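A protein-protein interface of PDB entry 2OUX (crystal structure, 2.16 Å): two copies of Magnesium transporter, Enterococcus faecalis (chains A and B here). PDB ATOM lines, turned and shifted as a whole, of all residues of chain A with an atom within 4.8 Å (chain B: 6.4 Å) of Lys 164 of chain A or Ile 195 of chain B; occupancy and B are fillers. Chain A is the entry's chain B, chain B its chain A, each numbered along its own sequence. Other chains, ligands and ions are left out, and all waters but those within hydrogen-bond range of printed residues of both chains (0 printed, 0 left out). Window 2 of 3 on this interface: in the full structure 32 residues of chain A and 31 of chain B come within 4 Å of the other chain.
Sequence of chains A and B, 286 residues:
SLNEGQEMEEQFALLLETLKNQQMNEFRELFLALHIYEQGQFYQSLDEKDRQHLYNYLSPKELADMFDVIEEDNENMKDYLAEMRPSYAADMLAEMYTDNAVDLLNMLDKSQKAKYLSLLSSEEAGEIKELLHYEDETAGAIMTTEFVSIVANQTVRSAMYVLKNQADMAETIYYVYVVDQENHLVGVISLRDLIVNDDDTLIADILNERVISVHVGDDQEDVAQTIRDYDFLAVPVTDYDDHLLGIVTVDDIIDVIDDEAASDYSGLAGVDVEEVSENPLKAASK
The backbone carbonyl oxygen of Ala 167 of chain A lies within hydrogen-bond range of the guanidinium group of Arg 192 of chain B.
Among the printed residues, pairs that only touch across the chains: Ile 195 of chain A with Met 160 of chain B (3.2 Å), Lys 164 of chain A with Ile 195 of chain B (3.5 Å), Leu 191 of chain A with Leu 191 of chain B (3.6 Å), Ala 167 of chain A with Val 196 of chain B (3.6 Å) and Lys 164 of chain A with Val 196 of chain B (3.9 Å).
Of chain B, only Ile 195 and Val 196 come within 4 Å of Lys 164 of chain A. Of chain A, only Lys 164 comes within 4 Å of Ile 195 of chain B. Printed residues of chain A within 4 Å of Arg 192 of chain B: Ala 167. Of the printed residues of chain A, Val 196 of chain B touches Lys 164 and Ala 167. Of the printed residues of chain A, Met 160 of chain B touches Ile 195. Of the printed residues of chain A, Leu 191 of chain B touches Leu 191 (3.6 Å). Asn 165 of chain A touches none of the printed residues of chain B.
Of the 10 printed residues of chain B, 5 touch a printed residue of chain A. Hydrophobic or aromatic side chains of chain B that line the printed part of chain A: Met 160, Leu 191 and Val 196. Among the printed residues, 6 pairs touch across the chains. Among the printed residues, no Asp or Glu carboxylate lies within 4 Å of a Lys or Arg side-chain nitrogen of the other chain.
Leu 191 of chain A touches its own counterpart, Leu 191 of chain B. Ile 195 of chain A touches Met 160 of chain B, but with the chains exchanged Met 160 of chain A does not touch Ile 195 of chain B (4.1 Å).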
ATOM      1  N   MET A 160      17.901 -16.432 -33.324  1.00  0.00           N
ATOM      2  CA  MET A 160      18.405 -17.471 -32.435  1.00  0.00           C
ATOM      3  C   MET A 160      18.867 -18.681 -33.243  1.00  0.00           C
ATOM      4  O   MET A 160      19.918 -19.265 -32.965  1.00  0.00           O
ATOM      5  CB  MET A 160      17.328 -17.893 -31.430  1.00  0.00           C
ATOM      6  CG  MET A 160      17.110 -16.904 -30.283  1.00  0.00           C
ATOM      7  SD  MET A 160      18.726 -16.488 -29.242  1.00  0.00           S
ATOM      8  CE  MET A 160      19.117 -18.255 -28.549  1.00  0.00           C
ATOM      9  N   TYR A 161      18.084 -19.050 -34.250  1.00  0.00           N
ATOM     10  CA  TYR A 161      18.438 -20.183 -35.086  1.00  0.00           C
ATOM     11  C   TYR A 161      19.852 -19.977 -35.645  1.00  0.00           C
ATOM     12  O   TYR A 161      20.696 -20.869 -35.571  1.00  0.00           O
ATOM     13  CB  TYR A 161      17.426 -20.324 -36.225  1.00  0.00           C
ATOM     14  CG  TYR A 161      17.642 -21.535 -37.094  1.00  0.00           C
ATOM     15  CD1 TYR A 161      17.362 -22.819 -36.620  1.00  0.00           C
ATOM     16  CD2 TYR A 161      18.147 -21.405 -38.388  1.00  0.00           C
ATOM     17  CE1 TYR A 161      17.579 -23.946 -37.421  1.00  0.00           C
ATOM     18  CE2 TYR A 161      18.368 -22.526 -39.198  1.00  0.00           C
ATOM     19  CZ  TYR A 161      18.085 -23.789 -38.710  1.00  0.00           C
ATOM     20  OH  TYR A 161      18.299 -24.888 -39.511  1.00  0.00           O
ATOM     21  N   VAL A 162      20.110 -18.794 -36.191  1.00  0.00           N
ATOM     22  CA  VAL A 162      21.421 -18.476 -36.749  1.00  0.00           C
ATOM     23  C   VAL A 162      22.507 -18.523 -35.679  1.00  0.00           C
ATOM     24  O   VAL A 162      23.600 -19.039 -35.913  1.00  0.00           O
ATOM     25  CB  VAL A 162      21.427 -17.071 -37.386  1.00  0.00           C
ATOM     26  CG1 VAL A 162      22.838 -16.703 -37.851  1.00  0.00           C
ATOM     27  CG2 VAL A 162      20.466 -17.040 -38.558  1.00  0.00           C
ATOM     28  N   LEU A 163      22.193 -17.974 -34.510  1.00  0.00           N
ATOM     29  CA  LEU A 163      23.125 -17.935 -33.391  1.00  0.00           C
ATOM     30  C   LEU A 163      23.612 -19.310 -32.981  1.00  0.00           C
ATOM     31  O   LEU A 163      24.813 -19.531 -32.825  1.00  0.00           O
ATOM     32  CB  LEU A 163      22.472 -17.251 -32.191  1.00  0.00           C
ATOM     33  CG  LEU A 163      22.705 -15.746 -32.028  1.00  0.00           C
ATOM     34  CD1 LEU A 163      24.118 -15.515 -31.545  1.00  0.00           C
ATOM     35  CD2 LEU A 163      22.456 -15.014 -33.336  1.00  0.00           C
ATOM     36  N   LYS A 164      22.680 -20.238 -32.808  1.00  0.00           N
ATOM     37  CA  LYS A 164      23.037 -21.592 -32.412  1.00  0.00           C
ATOM     38  C   LYS A 164      23.990 -22.236 -33.414  1.00  0.00           C
ATOM     39  O   LYS A 164      24.956 -22.894 -33.025  1.00  0.00           O
ATOM     40  CB  LYS A 164      21.770 -22.436 -32.261  1.00  0.00           C
ATOM     41  CG  LYS A 164      20.796 -21.865 -31.245  1.00  0.00           C
ATOM     42  CD  LYS A 164      19.582 -22.758 -31.095  1.00  0.00           C
ATOM     43  CE  LYS A 164      18.568 -22.174 -30.125  1.00  0.00           C
ATOM     44  NZ  LYS A 164      17.322 -23.007 -30.070  1.00  0.00           N
ATOM     45  N   ASN A 165      23.713 -22.040 -34.701  1.00  0.00           N
ATOM     46  CA  ASN A 165      24.546 -22.587 -35.771  1.00  0.00           C
ATOM     47  C   ASN A 165      25.958 -21.986 -35.799  1.00  0.00           C
ATOM     48  O   ASN A 165      26.907 -22.641 -36.237  1.00  0.00           O
ATOM     49  CB  ASN A 165      23.876 -22.349 -37.130  1.00  0.00           C
ATOM     50  CG  ASN A 165      22.687 -23.270 -37.375  1.00  0.00           C
ATOM     51  OD1 ASN A 165      21.882 -23.036 -38.283  1.00  0.00           O
ATOM     52  ND2 ASN A 165      22.579 -24.328 -36.576  1.00  0.00           N
ATOM     53  N   GLN A 166      26.092 -20.745 -35.333  1.00  0.00           N
ATOM     54  CA  GLN A 166      27.381 -20.052 -35.313  1.00  0.00           C
ATOM     55  C   GLN A 166      28.168 -20.209 -34.022  1.00  0.00           C
ATOM     56  O   GLN A 166      29.361 -19.933 -33.990  1.00  0.00           O
ATOM     57  CB  GLN A 166      27.180 -18.556 -35.578  1.00  0.00           C
ATOM     58  CG  GLN A 166      26.798 -18.226 -37.005  1.00  0.00           C
ATOM     59  CD  GLN A 166      27.953 -18.431 -37.966  1.00  0.00           C
ATOM     60  OE1 GLN A 166      28.875 -17.619 -38.032  1.00  0.00           O
ATOM     61  NE2 GLN A 166      27.913 -19.530 -38.708  1.00  0.00           N
ATOM     62  N   ALA A 167      27.501 -20.631 -32.955  1.00  0.00           N
ATOM     63  CA  ALA A 167      28.150 -20.800 -31.658  1.00  0.00           C
ATOM     64  C   ALA A 167      29.542 -21.414 -31.756  1.00  0.00           C
ATOM     65  O   ALA A 167      30.523 -20.833 -31.293  1.00  0.00           O
ATOM     66  CB  ALA A 167      27.279 -21.656 -30.756  1.00  0.00           C
ATOM     67  N   ASP A 168      29.615 -22.589 -32.374  1.00  0.00           N
ATOM     68  CA  ASP A 168      30.864 -23.324 -32.536  1.00  0.00           C
ATOM     69  C   ASP A 168      31.971 -22.635 -33.335  1.00  0.00           C
ATOM     70  O   ASP A 168      33.157 -22.852 -33.064  1.00  0.00           O
ATOM     71  CB  ASP A 168      30.578 -24.697 -33.162  1.00  0.00           C
ATOM     72  CG  ASP A 168      29.401 -24.668 -34.135  1.00  0.00           C
ATOM     73  OD1 ASP A 168      29.229 -23.652 -34.849  1.00  0.00           O
ATOM     74  OD2 ASP A 168      28.650 -25.671 -34.189  1.00  0.00           O
ATOM     75  N   LEU A 191      23.051 -10.669 -27.391  1.00  0.00           N
ATOM     76  CA  LEU A 191      22.347 -11.931 -27.191  1.00  0.00           C
ATOM     77  C   LEU A 191      21.440 -11.774 -25.978  1.00  0.00           C
ATOM     78  O   LEU A 191      20.366 -12.384 -25.902  1.00  0.00           O
ATOM     79  CB  LEU A 191      23.330 -13.090 -26.966  1.00  0.00           C
ATOM     80  CG  LEU A 191      22.705 -14.414 -26.490  1.00  0.00           C
ATOM     81  CD1 LEU A 191      21.597 -14.870 -27.456  1.00  0.00           C
ATOM     82  CD2 LEU A 191      23.785 -15.477 -26.363  1.00  0.00           C
ATOM     83  N   ILE A 195      17.517 -12.958 -25.924  1.00  0.00           N
ATOM     84  CA  ILE A 195      16.985 -13.899 -24.950  1.00  0.00           C
ATOM     85  C   ILE A 195      15.739 -13.448 -24.178  1.00  0.00           C
ATOM     86  O   ILE A 195      14.887 -14.277 -23.854  1.00  0.00           O
ATOM     87  CB  ILE A 195      18.100 -14.324 -23.936  1.00  0.00           C
ATOM     88  CG1 ILE A 195      18.927 -15.471 -24.529  1.00  0.00           C
ATOM     89  CG2 ILE A 195      17.483 -14.708 -22.588  1.00  0.00           C
ATOM     90  CD1 ILE A 195      18.081 -16.647 -24.978  1.00  0.00           C
ATOM     91  N   MET B 160      17.142 -21.414 -18.552  1.00  0.00           N
ATOM     92  CA  MET B 160      16.793 -20.415 -19.556  1.00  0.00           C
ATOM     93  C   MET B 160      15.592 -19.577 -19.145  1.00  0.00           C
ATOM     94  O   MET B 160      15.373 -18.490 -19.687  1.00  0.00           O
ATOM     95  CB  MET B 160      16.498 -21.090 -20.897  1.00  0.00           C
ATOM     96  CG  MET B 160      17.725 -21.626 -21.634  1.00  0.00           C
ATOM     97  SD  MET B 160      18.969 -20.234 -22.223  1.00  0.00           S
ATOM     98  CE  MET B 160      17.674 -18.887 -22.687  1.00  0.00           C
ATOM     99  N   SER B 190      28.882 -21.488 -19.969  1.00  0.00           N
ATOM    100  CA  SER B 190      28.758 -20.236 -20.706  1.00  0.00           C
ATOM    101  C   SER B 190      27.391 -20.214 -21.365  1.00  0.00           C
ATOM    102  O   SER B 190      26.816 -21.264 -21.651  1.00  0.00           O
ATOM    103  CB  SER B 190      29.832 -20.134 -21.786  1.00  0.00           C
ATOM    104  OG  SER B 190      29.621 -21.127 -22.772  1.00  0.00           O
ATOM    105  N   LEU B 191      26.864 -19.024 -21.608  1.00  0.00           N
ATOM    106  CA  LEU B 191      25.557 -18.935 -22.232  1.00  0.00           C
ATOM    107  C   LEU B 191      25.604 -19.526 -23.643  1.00  0.00           C
ATOM    108  O   LEU B 191      24.645 -20.162 -24.093  1.00  0.00           O
ATOM    109  CB  LEU B 191      25.079 -17.483 -22.292  1.00  0.00           C
ATOM    110  CG  LEU B 191      23.669 -17.341 -22.872  1.00  0.00           C
ATOM    111  CD1 LEU B 191      22.692 -18.203 -22.060  1.00  0.00           C
ATOM    112  CD2 LEU B 191      23.250 -15.885 -22.843  1.00  0.00           C
ATOM    113  N   ARG B 192      26.727 -19.329 -24.329  1.00  0.00           N
ATOM    114  CA  ARG B 192      26.873 -19.851 -25.679  1.00  0.00           C
ATOM    115  C   ARG B 192      26.858 -21.382 -25.740  1.00  0.00           C
ATOM    116  O   ARG B 192      26.546 -21.952 -26.779  1.00  0.00           O
ATOM    117  CB  ARG B 192      28.146 -19.306 -26.340  1.00  0.00           C
ATOM    118  CG  ARG B 192      29.476 -19.769 -25.745  1.00  0.00           C
ATOM    119  CD  ARG B 192      30.660 -19.034 -26.416  1.00  0.00           C
ATOM    120  NE  ARG B 192      30.803 -19.365 -27.833  1.00  0.00           N
ATOM    121  CZ  ARG B 192      31.562 -18.693 -28.696  1.00  0.00           C
ATOM    122  NH1 ARG B 192      32.262 -17.638 -28.299  1.00  0.00           N
ATOM    123  NH2 ARG B 192      31.620 -19.075 -29.961  1.00  0.00           N
ATOM    124  N   ASP B 193      27.201 -22.047 -24.643  1.00  0.00           N
ATOM    125  CA  ASP B 193      27.173 -23.510 -24.619  1.00  0.00           C
ATOM    126  C   ASP B 193      25.767 -23.921 -24.249  1.00  0.00           C
ATOM    127  O   ASP B 193      25.239 -24.930 -24.720  1.00  0.00           O
ATOM    128  CB  ASP B 193      28.145 -24.071 -23.586  1.00  0.00           C
ATOM    129  CG  ASP B 193      29.566 -24.071 -24.076  1.00  0.00           C
ATOM    130  OD1 ASP B 193      29.764 -23.908 -25.294  1.00  0.00           O
ATOM    131  OD2 ASP B 193      30.484 -24.247 -23.253  1.00  0.00           O
ATOM    132  N   LEU B 194      25.163 -23.102 -23.403  1.00  0.00           N
ATOM    133  CA  LEU B 194      23.812 -23.334 -22.936  1.00  0.00           C
ATOM    134  C   LEU B 194      22.776 -23.308 -24.058  1.00  0.00           C
ATOM    135  O   LEU B 194      22.028 -24.268 -24.236  1.00  0.00           O
ATOM    136  CB  LEU B 194      23.451 -22.283 -21.886  1.00  0.00           C
ATOM    137  CG  LEU B 194      22.194 -22.518 -21.054  1.00  0.00           C
ATOM    138  CD1 LEU B 194      22.330 -23.822 -20.268  1.00  0.00           C
ATOM    139  CD2 LEU B 194      22.001 -21.352 -20.092  1.00  0.00           C
ATOM    140  N   ILE B 195      22.732 -22.222 -24.822  1.00  0.00           N
ATOM    141  CA  ILE B 195      21.735 -22.098 -25.879  1.00  0.00           C
ATOM    142  C   ILE B 195      21.738 -23.173 -26.960  1.00  0.00           C
ATOM    143  O   ILE B 195      20.742 -23.320 -27.682  1.00  0.00           O
ATOM    144  CB  ILE B 195      21.807 -20.720 -26.580  1.00  0.00           C
ATOM    145  CG1 ILE B 195      23.113 -20.589 -27.366  1.00  0.00           C
ATOM    146  CG2 ILE B 195      21.677 -19.611 -25.550  1.00  0.00           C
ATOM    147  CD1 ILE B 195      23.109 -19.424 -28.333  1.00  0.00           C
ATOM    148  N   VAL B 196      22.828 -23.924 -27.089  1.00  0.00           N
ATOM    149  CA  VAL B 196      22.873 -24.963 -28.114  1.00  0.00           C
ATOM    150  C   VAL B 196      22.503 -26.332 -27.546  1.00  0.00           C
ATOM    151  O   VAL B 196      22.715 -27.354 -28.191  1.00  0.00           O
ATOM    152  CB  VAL B 196      24.270 -25.082 -28.765  1.00  0.00           C
ATOM    153  CG1 VAL B 196      24.776 -23.703 -29.184  1.00  0.00           C
ATOM    154  CG2 VAL B 196      25.237 -25.765 -27.810  1.00  0.00           C
ATOM    155  N   ASN B 197      21.962 -26.359 -26.335  1.00  0.00           N
ATOM    156  CA  ASN B 197      21.586 -27.629 -25.737  1.00  0.00           C
ATOM    157  C   ASN B 197      20.071 -27.788 -25.717  1.00  0.00           C
ATOM    158  O   ASN B 197      19.332 -26.800 -25.751  1.00  0.00           O
ATOM    159  CB  ASN B 197      22.176 -27.744 -24.328  1.00  0.00           C
ATOM    160  CG  ASN B 197      23.556 -28.379 -24.330  1.00  0.00           C
ATOM    161  OD1 ASN B 197      23.686 -29.602 -24.391  1.00  0.00           O
ATOM    162  ND2 ASN B 197      24.596 -27.549 -24.285  1.00  0.00           N
ATOM    163  N   ASP B 198      19.609 -29.032 -25.672  1.00  0.00           N
ATOM    164  CA  ASP B 198      18.177 -29.298 -25.669  1.00  0.00           C
ATOM    165  C   ASP B 198      17.494 -28.866 -24.384  1.00  0.00           C
ATOM    166  O   ASP B 198      18.077 -28.931 -23.308  1.00  0.00           O
ATOM    167  CB  ASP B 198      17.891 -30.782 -25.892  1.00  0.00           C
ATOM    168  CG  ASP B 198      16.404 -31.062 -26.012  1.00  0.00           C
ATOM    169  OD1 ASP B 198      15.825 -30.729 -27.066  1.00  0.00           O
ATOM    170  OD2 ASP B 198      15.808 -31.587 -25.047  1.00  0.00           O
